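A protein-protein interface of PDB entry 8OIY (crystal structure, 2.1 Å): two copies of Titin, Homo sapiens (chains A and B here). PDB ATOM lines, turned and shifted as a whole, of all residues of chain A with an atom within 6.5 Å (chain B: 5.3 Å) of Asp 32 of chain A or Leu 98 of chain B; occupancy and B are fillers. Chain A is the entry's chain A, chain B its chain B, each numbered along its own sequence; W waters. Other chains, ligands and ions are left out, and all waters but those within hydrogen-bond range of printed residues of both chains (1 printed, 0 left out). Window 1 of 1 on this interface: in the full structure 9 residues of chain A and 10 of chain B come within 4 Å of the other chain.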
ATOM      1  N   GLU A   4      -4.354  20.110  33.154  1.00  0.00           N
ATOM      2  CA  GLU A   4      -4.816  18.729  33.157  1.00  0.00           C
ATOM      3  C   GLU A   4      -5.192  18.308  31.743  1.00  0.00           C
ATOM      4  O   GLU A   4      -5.264  19.124  30.820  1.00  0.00           O
ATOM      5  CB  GLU A   4      -6.002  18.547  34.111  1.00  0.00           C
ATOM      6  CG  GLU A   4      -7.041  19.653  34.032  1.00  0.00           C
ATOM      7  CD  GLU A   4      -8.359  19.260  34.670  1.00  0.00           C
ATOM      8  OE1 GLU A   4      -8.340  18.477  35.646  1.00  0.00           O
ATOM      9  OE2 GLU A   4      -9.414  19.730  34.195  1.00  0.00           O
ATOM     10  N   ARG A   5      -5.426  17.007  31.585  1.00  0.00           N
ATOM     11  CA  ARG A   5      -5.751  16.448  30.283  1.00  0.00           C
ATOM     12  C   ARG A   5      -7.078  17.011  29.774  1.00  0.00           C
ATOM     13  O   ARG A   5      -7.940  17.404  30.563  1.00  0.00           O
ATOM     14  CB  ARG A   5      -5.843  14.926  30.373  1.00  0.00           C
ATOM     15  CG  ARG A   5      -6.838  14.443  31.419  1.00  0.00           C
ATOM     16  CD  ARG A   5      -7.099  12.952  31.320  1.00  0.00           C
ATOM     17  NE  ARG A   5      -8.226  12.556  32.159  1.00  0.00           N
ATOM     18  CZ  ARG A   5      -8.129  12.203  33.435  1.00  0.00           C
ATOM     19  NH1 ARG A   5      -6.962  12.168  34.057  1.00  0.00           N
ATOM     20  NH2 ARG A   5      -9.232  11.880  34.104  1.00  0.00           N
ATOM     21  N   PRO A   6      -7.272  17.053  28.460  1.00  0.00           N
ATOM     22  CA  PRO A   6      -8.552  17.511  27.915  1.00  0.00           C
ATOM     23  C   PRO A   6      -9.602  16.410  27.983  1.00  0.00           C
ATOM     24  O   PRO A   6      -9.318  15.252  28.291  1.00  0.00           O
ATOM     25  CB  PRO A   6      -8.211  17.867  26.464  1.00  0.00           C
ATOM     26  CG  PRO A   6      -7.094  16.950  26.115  1.00  0.00           C
ATOM     27  CD  PRO A   6      -6.329  16.663  27.394  1.00  0.00           C
ATOM     28  N   SER A   7     -10.838  16.800  27.697  1.00  0.00           N
ATOM     29  CA  SER A   7     -11.935  15.852  27.590  1.00  0.00           C
ATOM     30  C   SER A   7     -11.848  15.130  26.251  1.00  0.00           C
ATOM     31  O   SER A   7     -11.069  15.510  25.374  1.00  0.00           O
ATOM     32  CB  SER A   7     -13.265  16.580  27.752  1.00  0.00           C
ATOM     33  OG  SER A   7     -13.406  17.610  26.792  1.00  0.00           O
ATOM     34  N   PRO A  29     -12.426  18.571  21.741  1.00  0.00           N
ATOM     35  CA  PRO A  29     -12.964  18.389  23.095  1.00  0.00           C
ATOM     36  C   PRO A  29     -13.824  19.567  23.526  1.00  0.00           C
ATOM     37  O   PRO A  29     -13.600  20.708  23.118  1.00  0.00           O
ATOM     38  CB  PRO A  29     -11.705  18.271  23.963  1.00  0.00           C
ATOM     39  CG  PRO A  29     -10.663  17.740  23.037  1.00  0.00           C
ATOM     40  CD  PRO A  29     -10.968  18.342  21.688  1.00  0.00           C
ATOM     41  N   LEU A  30     -14.823  19.274  24.362  1.00  0.00           N
ATOM     42  CA  LEU A  30     -15.601  20.335  24.988  1.00  0.00           C
ATOM     43  C   LEU A  30     -14.789  21.077  26.042  1.00  0.00           C
ATOM     44  O   LEU A  30     -15.106  22.228  26.361  1.00  0.00           O
ATOM     45  CB  LEU A  30     -16.869  19.762  25.624  1.00  0.00           C
ATOM     46  CG  LEU A  30     -17.908  19.096  24.714  1.00  0.00           C
ATOM     47  CD1 LEU A  30     -19.172  18.794  25.514  1.00  0.00           C
ATOM     48  CD2 LEU A  30     -18.249  19.943  23.502  1.00  0.00           C
ATOM     49  N   LYS A  31     -13.752  20.441  26.584  1.00  0.00           N
ATOM     50  CA  LYS A  31     -12.915  21.024  27.628  1.00  0.00           C
ATOM     51  C   LYS A  31     -11.469  20.656  27.334  1.00  0.00           C
ATOM     52  O   LYS A  31     -11.143  19.469  27.220  1.00  0.00           O
ATOM     53  CB  LYS A  31     -13.329  20.519  29.014  1.00  0.00           C
ATOM     54  CG  LYS A  31     -14.830  20.563  29.268  1.00  0.00           C
ATOM     55  CD  LYS A  31     -15.219  19.798  30.525  1.00  0.00           C
ATOM     56  CE  LYS A  31     -16.668  20.070  30.906  1.00  0.00           C
ATOM     57  NZ  LYS A  31     -17.617  19.633  29.840  1.00  0.00           N
ATOM     58  N   ASP A  32     -10.606  21.662  27.210  1.00  0.00           N
ATOM     59  CA  ASP A  32      -9.205  21.425  26.888  1.00  0.00           C
ATOM     60  C   ASP A  32      -8.330  21.270  28.125  1.00  0.00           C
ATOM     61  O   ASP A  32      -7.111  21.117  27.990  1.00  0.00           O
ATOM     62  CB  ASP A  32      -8.664  22.557  26.003  1.00  0.00           C
ATOM     63  CG  ASP A  32      -8.775  23.924  26.656  1.00  0.00           C
ATOM     64  OD1 ASP A  32      -8.988  23.996  27.885  1.00  0.00           O
ATOM     65  OD2 ASP A  32      -8.644  24.931  25.928  1.00  0.00           O
ATOM     66  N   GLY A  33      -8.917  21.303  29.321  1.00  0.00           N
ATOM     67  CA  GLY A  33      -8.160  21.107  30.539  1.00  0.00           C
ATOM     68  C   GLY A  33      -7.259  22.253  30.929  1.00  0.00           C
ATOM     69  O   GLY A  33      -6.428  22.089  31.829  1.00  0.00           O
ATOM     70  N   GLY A  34      -7.393  23.407  30.287  1.00  0.00           N
ATOM     71  CA  GLY A  34      -6.570  24.552  30.590  1.00  0.00           C
ATOM     72  C   GLY A  34      -5.367  24.748  29.696  1.00  0.00           C
ATOM     73  O   GLY A  34      -4.566  25.651  29.961  1.00  0.00           O
ATOM     74  N   SER A  35      -5.210  23.941  28.652  1.00  0.00           N
ATOM     75  CA  SER A  35      -4.073  24.067  27.750  1.00  0.00           C
ATOM     76  C   SER A  35      -4.509  23.686  26.344  1.00  0.00           C
ATOM     77  O   SER A  35      -5.345  22.789  26.180  1.00  0.00           O
ATOM     78  CB  SER A  35      -2.901  23.184  28.203  1.00  0.00           C
ATOM     79  OG  SER A  35      -1.763  23.402  27.389  1.00  0.00           O
ATOM     80  N   PRO A  36      -3.962  24.338  25.315  1.00  0.00           N
ATOM     81  CA  PRO A  36      -4.410  24.059  23.944  1.00  0.00           C
ATOM     82  C   PRO A  36      -4.192  22.608  23.538  1.00  0.00           C
ATOM     83  O   PRO A  36      -3.310  21.917  24.052  1.00  0.00           O
ATOM     84  CB  PRO A  36      -3.551  25.003  23.091  1.00  0.00           C
ATOM     85  CG  PRO A  36      -3.155  26.094  24.012  1.00  0.00           C
ATOM     86  CD  PRO A  36      -2.999  25.455  25.362  1.00  0.00           C
ATOM     87  N   ILE A  37      -5.008  22.156  22.587  1.00  0.00           N
ATOM     88  CA  ILE A  37      -4.875  20.812  22.033  1.00  0.00           C
ATOM     89  C   ILE A  37      -3.716  20.806  21.045  1.00  0.00           C
ATOM     90  O   ILE A  37      -3.724  21.546  20.055  1.00  0.00           O
ATOM     91  CB  ILE A  37      -6.172  20.359  21.349  1.00  0.00           C
ATOM     92  CG1 ILE A  37      -7.365  20.490  22.296  1.00  0.00           C
ATOM     93  CG2 ILE A  37      -6.024  18.925  20.837  1.00  0.00           C
ATOM     94  CD1 ILE A  37      -7.234  19.703  23.577  1.00  0.00           C
ATOM     95  N   ASN A  84      -2.824  17.447  25.038  1.00  0.00           N
ATOM     96  CA  ASN A  84      -2.271  18.771  25.295  1.00  0.00           C
ATOM     97  C   ASN A  84      -0.977  18.613  26.085  1.00  0.00           C
ATOM     98  O   ASN A  84      -0.503  17.490  26.290  1.00  0.00           O
ATOM     99  CB  ASN A  84      -3.273  19.650  26.047  1.00  0.00           C
ATOM    100  CG  ASN A  84      -3.664  19.080  27.400  1.00  0.00           C
ATOM    101  OD1 ASN A  84      -3.078  18.110  27.876  1.00  0.00           O
ATOM    102  ND2 ASN A  84      -4.669  19.685  28.024  1.00  0.00           N
ATOM    103  N   ALA A  86      -0.557  18.715  29.087  1.00  0.00           N
ATOM    104  CA  ALA A  86      -0.787  18.033  30.354  1.00  0.00           C
ATOM    105  C   ALA A  86      -0.931  16.526  30.203  1.00  0.00           C
ATOM    106  O   ALA A  86      -0.572  15.786  31.127  1.00  0.00           O
ATOM    107  CB  ALA A  86      -2.039  18.599  31.033  1.00  0.00           C
ATOM    108  N   SER B  14     -16.298  24.349  18.390  1.00  0.00           N
ATOM    109  CA  SER B  14     -15.361  25.451  18.234  1.00  0.00           C
ATOM    110  C   SER B  14     -14.312  25.117  17.185  1.00  0.00           C
ATOM    111  O   SER B  14     -14.138  23.961  16.791  1.00  0.00           O
ATOM    112  CB  SER B  14     -14.665  25.783  19.564  1.00  0.00           C
ATOM    113  OG  SER B  14     -13.954  24.658  20.052  1.00  0.00           O
ATOM    114  N   GLN B  17      -9.153  28.531  17.414  1.00  0.00           N
ATOM    115  CA  GLN B  17      -8.835  29.147  18.697  1.00  0.00           C
ATOM    116  C   GLN B  17      -7.523  29.915  18.594  1.00  0.00           C
ATOM    117  O   GLN B  17      -6.497  29.365  18.175  1.00  0.00           O
ATOM    118  CB  GLN B  17      -8.744  28.085  19.793  1.00  0.00           C
ATOM    119  CG  GLN B  17      -8.385  28.631  21.177  1.00  0.00           C
ATOM    120  CD  GLN B  17      -9.523  29.406  21.820  1.00  0.00           C
ATOM    121  OE1 GLN B  17     -10.516  28.828  22.255  1.00  0.00           O
ATOM    122  NE2 GLN B  17      -9.379  30.724  21.881  1.00  0.00           N
ATOM    123  N   VAL B  22     -12.111  33.049  18.975  1.00  0.00           N
ATOM    124  CA  VAL B  22     -12.440  31.656  18.706  1.00  0.00           C
ATOM    125  C   VAL B  22     -13.663  31.643  17.802  1.00  0.00           C
ATOM    126  O   VAL B  22     -14.542  32.502  17.909  1.00  0.00           O
ATOM    127  CB  VAL B  22     -12.687  30.866  20.016  1.00  0.00           C
ATOM    128  CG1 VAL B  22     -13.921  31.388  20.735  1.00  0.00           C
ATOM    129  CG2 VAL B  22     -12.824  29.376  19.712  1.00  0.00           C
ATOM    130  N   ASN B  74      -6.678  33.082  29.485  1.00  0.00           N
ATOM    131  CA  ASN B  74      -7.894  32.853  30.246  1.00  0.00           C
ATOM    132  C   ASN B  74      -8.703  31.697  29.660  1.00  0.00           C
ATOM    133  O   ASN B  74      -8.574  31.338  28.485  1.00  0.00           O
ATOM    134  CB  ASN B  74      -8.748  34.122  30.277  1.00  0.00           C
ATOM    135  CG  ASN B  74      -8.194  35.173  31.218  1.00  0.00           C
ATOM    136  OD1 ASN B  74      -8.479  35.158  32.416  1.00  0.00           O
ATOM    137  ND2 ASN B  74      -7.398  36.091  30.681  1.00  0.00           N
ATOM    138  N   LYS B  75      -9.547  31.112  30.510  1.00  0.00           N
ATOM    139  CA  LYS B  75     -10.452  30.035  30.126  1.00  0.00           C
ATOM    140  C   LYS B  75     -11.868  30.585  30.011  1.00  0.00           C
ATOM    141  O   LYS B  75     -12.287  31.417  30.821  1.00  0.00           O
ATOM    142  CB  LYS B  75     -10.417  28.899  31.150  1.00  0.00           C
ATOM    143  CG  LYS B  75      -9.235  27.950  30.999  1.00  0.00           C
ATOM    144  CD  LYS B  75      -7.912  28.658  31.243  1.00  0.00           C
ATOM    145  N   TYR B  76     -12.606  30.112  29.009  1.00  0.00           N
ATOM    146  CA  TYR B  76     -13.921  30.656  28.697  1.00  0.00           C
ATOM    147  C   TYR B  76     -14.939  29.546  28.497  1.00  0.00           C
ATOM    148  O   TYR B  76     -14.616  28.476  27.973  1.00  0.00           O
ATOM    149  CB  TYR B  76     -13.864  31.531  27.436  1.00  0.00           C
ATOM    150  CG  TYR B  76     -13.000  32.764  27.589  1.00  0.00           C
ATOM    151  CD1 TYR B  76     -11.638  32.718  27.328  1.00  0.00           C
ATOM    152  CD2 TYR B  76     -13.549  33.970  27.997  1.00  0.00           C
ATOM    153  CE1 TYR B  76     -10.845  33.841  27.468  1.00  0.00           C
ATOM    154  CE2 TYR B  76     -12.766  35.100  28.138  1.00  0.00           C
ATOM    155  CZ  TYR B  76     -11.415  35.029  27.874  1.00  0.00           C
ATOM    156  OH  TYR B  76     -10.631  36.149  28.015  1.00  0.00           O
ATOM    157  N   LEU B  77     -16.171  29.814  28.923  1.00  0.00           N
ATOM    158  CA  LEU B  77     -17.327  28.986  28.620  1.00  0.00           C
ATOM    159  C   LEU B  77     -18.179  29.685  27.568  1.00  0.00           C
ATOM    160  O   LEU B  77     -18.160  30.915  27.453  1.00  0.00           O
ATOM    161  CB  LEU B  77     -18.165  28.721  29.872  1.00  0.00           C
ATOM    162  CG  LEU B  77     -17.442  28.109  31.074  1.00  0.00           C
ATOM    163  CD1 LEU B  77     -18.287  28.246  32.335  1.00  0.00           C
ATOM    164  CD2 LEU B  77     -17.109  26.655  30.813  1.00  0.00           C
ATOM    165  N   TYR B  78     -18.933  28.899  26.803  1.00  0.00           N
ATOM    166  CA  TYR B  78     -19.761  29.445  25.737  1.00  0.00           C
ATOM    167  C   TYR B  78     -21.093  28.715  25.684  1.00  0.00           C
ATOM    168  O   TYR B  78     -21.185  27.524  26.000  1.00  0.00           O
ATOM    169  CB  TYR B  78     -19.069  29.346  24.368  1.00  0.00           C
ATOM    170  CG  TYR B  78     -17.712  30.009  24.308  1.00  0.00           C
ATOM    171  CD1 TYR B  78     -17.594  31.374  24.087  1.00  0.00           C
ATOM    172  CD2 TYR B  78     -16.547  29.266  24.472  1.00  0.00           C
ATOM    173  CE1 TYR B  78     -16.351  31.985  24.033  1.00  0.00           C
ATOM    174  CE2 TYR B  78     -15.305  29.866  24.419  1.00  0.00           C
ATOM    175  CZ  TYR B  78     -15.212  31.225  24.200  1.00  0.00           C
ATOM    176  OH  TYR B  78     -13.971  31.821  24.147  1.00  0.00           O
ATOM    177  N   LEU B  95     -20.292  24.922  26.144  1.00  0.00           N
ATOM    178  CA  LEU B  95     -18.996  24.575  25.584  1.00  0.00           C
ATOM    179  C   LEU B  95     -17.903  25.221  26.424  1.00  0.00           C
ATOM    180  O   LEU B  95     -18.009  26.392  26.804  1.00  0.00           O
ATOM    181  CB  LEU B  95     -18.889  25.037  24.131  1.00  0.00           C
ATOM    182  CG  LEU B  95     -17.625  24.651  23.365  1.00  0.00           C
ATOM    183  CD1 LEU B  95     -17.551  23.147  23.165  1.00  0.00           C
ATOM    184  CD2 LEU B  95     -17.577  25.369  22.023  1.00  0.00           C
ATOM    185  N   GLY B  96     -16.857  24.451  26.720  1.00  0.00           N
ATOM    186  CA  GLY B  96     -15.752  24.942  27.507  1.00  0.00           C
ATOM    187  C   GLY B  96     -15.693  24.293  28.875  1.00  0.00           C
ATOM    188  O   GLY B  96     -16.544  23.475  29.232  1.00  0.00           O
ATOM    189  N   PRO B  97     -14.695  24.669  29.691  1.00  0.00           N
ATOM    190  CA  PRO B  97     -13.701  25.737  29.489  1.00  0.00           C
ATOM    191  C   PRO B  97     -12.752  25.527  28.311  1.00  0.00           C
ATOM    192  O   PRO B  97     -12.181  24.450  28.139  1.00  0.00           O
ATOM    193  CB  PRO B  97     -12.913  25.741  30.819  1.00  0.00           C
ATOM    194  CG  PRO B  97     -13.796  25.034  31.814  1.00  0.00           C
ATOM    195  CD  PRO B  97     -14.546  24.018  31.003  1.00  0.00           C
ATOM    196  N   LEU B  98     -12.582  26.559  27.485  1.00  0.00           N
ATOM    197  CA  LEU B  98     -11.628  26.563  26.383  1.00  0.00           C
ATOM    198  C   LEU B  98     -10.627  27.687  26.612  1.00  0.00           C
ATOM    199  O   LEU B  98     -11.020  28.841  26.815  1.00  0.00           O
ATOM    200  CB  LEU B  98     -12.331  26.754  25.034  1.00  0.00           C
ATOM    201  CG  LEU B  98     -13.351  25.694  24.614  1.00  0.00           C
ATOM    202  CD1 LEU B  98     -13.950  26.048  23.258  1.00  0.00           C
ATOM    203  CD2 LEU B  98     -12.722  24.312  24.581  1.00  0.00           C
ATOM    204  N   THR B  99      -9.341  27.351  26.575  1.00  0.00           N
ATOM    205  CA  THR B  99      -8.285  28.312  26.863  1.00  0.00           C
ATOM    206  C   THR B  99      -7.876  29.055  25.598  1.00  0.00           C
ATOM    207  O   THR B  99      -7.711  28.453  24.534  1.00  0.00           O
ATOM    208  CB  THR B  99      -7.068  27.608  27.469  1.00  0.00           C
ATOM    209  OG1 THR B  99      -7.489  26.744  28.532  1.00  0.00           O
ATOM    210  CG2 THR B  99      -6.074  28.626  28.008  1.00  0.00           C
ATOM    211  N   ALA B 100      -7.706  30.372  25.725  1.00  0.00           N
ATOM    212  CA  ALA B 100      -7.301  31.218  24.603  1.00  0.00           C
ATOM    213  C   ALA B 100      -5.777  31.222  24.522  1.00  0.00           C
ATOM    214  O   ALA B 100      -5.093  32.116  25.026  1.00  0.00           O
ATOM    215  CB  ALA B 100      -7.858  32.627  24.764  1.00  0.00           C
HETATM  216  O   HOH W   1     -18.323  22.038  28.018  1.00  0.00           O
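No position is printed for both chains.
Of the 11 pairs that touch across the chains among the printed residues, none has its exchanged pair printed and touching as well.
The backbone carbonyl oxygen (O) of Tyr 76 of chain B is in hydrogen-bond range of the backbone NH (N) of Leu 98 of chain B, 2.8 Å away.
The backbone NH of Gly 34 of chain A sits at hydrogen-bond distance from the side-chain carboxylate of Asp 32 of chain A (2.9 Å).
N of Tyr 78 of chain B is in hydrogen-bond range of O of Leu 95 of chain B, at 2.7 Å.
O of Asp 32 of chain A is in hydrogen-bond range of ND2 of Asn 84 of chain A (2.8 Å).
The backbone carbonyl oxygen (O) of Lys 31 of chain A lies within hydrogen-bond range of the backbone NH (N) of Ser 7 of chain A.
The side-chain hydroxyl (OG) of Ser 7 of chain A is in hydrogen-bond range of the backbone NH (N) of Leu 30 of chain A (3.3 Å).
The side-chain carboxylate of Asp 32 of chain A sits at hydrogen-bond distance from the backbone NH of Thr 99 of chain B, 2.6 Å away.
O of Leu 30 of chain A lies within hydrogen-bond range of N of Gly 96 of chain B (2.9 Å).
OG1 of Thr 99 of chain B sits close to O of Gly 34 of chain A.
N of Asp 32 of chain A is in hydrogen-bond range of O of Pro 97 of chain B (3.3 Å).
Of the printed residues of chain B, Pro 29 of chain A touches Leu 98 (3.99 Å).
Of chain B, only Pro 97, Leu 98 and Thr 99 come within 4 Å of Asp 32 of chain A.
Of the printed residues of chain B, Ser 35 of chain A touches Thr 99 (3.6 Å).
Of the printed residues of chain A, Leu 95 of chain B touches Leu 30 (3.3 Å).
Of the printed residues of chain A, Pro 97 of chain B touches Lys 31 and Asp 32.
The nearest residue of chain B that does not touch Asp 32 of chain A is Lys 75 of chain B (5.0 Å).
The nearest printed residue of chain B that does not touch Gly 34 of chain A is Lys 75 of chain B (4.3 Å).
Water W1 bridges the backbone carbonyl oxygen of Gly 96 of chain B and the side-chain amino group of Lys 31 of chain A.
Among the printed residues, merely in contact across the chains: Pro 29 of chain A with Leu 98 of chain B (3.99 Å), Leu 30 of chain A with Leu 95 of chain B (3.3 Å), Leu 30 of chain A with Leu 98 of chain B (3.6 Å), Lys 31 of chain A with Gly 96 of chain B (3.4 Å), Lys 31 of chain A with Pro 97 of chain B (3.5 Å), Asp 32 of chain A with Leu 98 of chain B (3.4 Å) and Ser 35 of chain A with Thr 99 of chain B (3.6 Å).
Of the 14 printed residues of chain B, 5 touch a printed residue of chain A.
Hydrophobic or aromatic side chains of chain B within 4 Å of the printed part of chain A: Leu 95, Pro 97 and Leu 98.
Of the 15 printed residues of chain A, 6 touch a printed residue of chain B.
Among the printed residues, 11 pairs touch across the chains.
Among the printed residues, no Asp or Glu carboxylate lies within 4 Å of a Lys or Arg side-chain nitrogen of the other chain.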
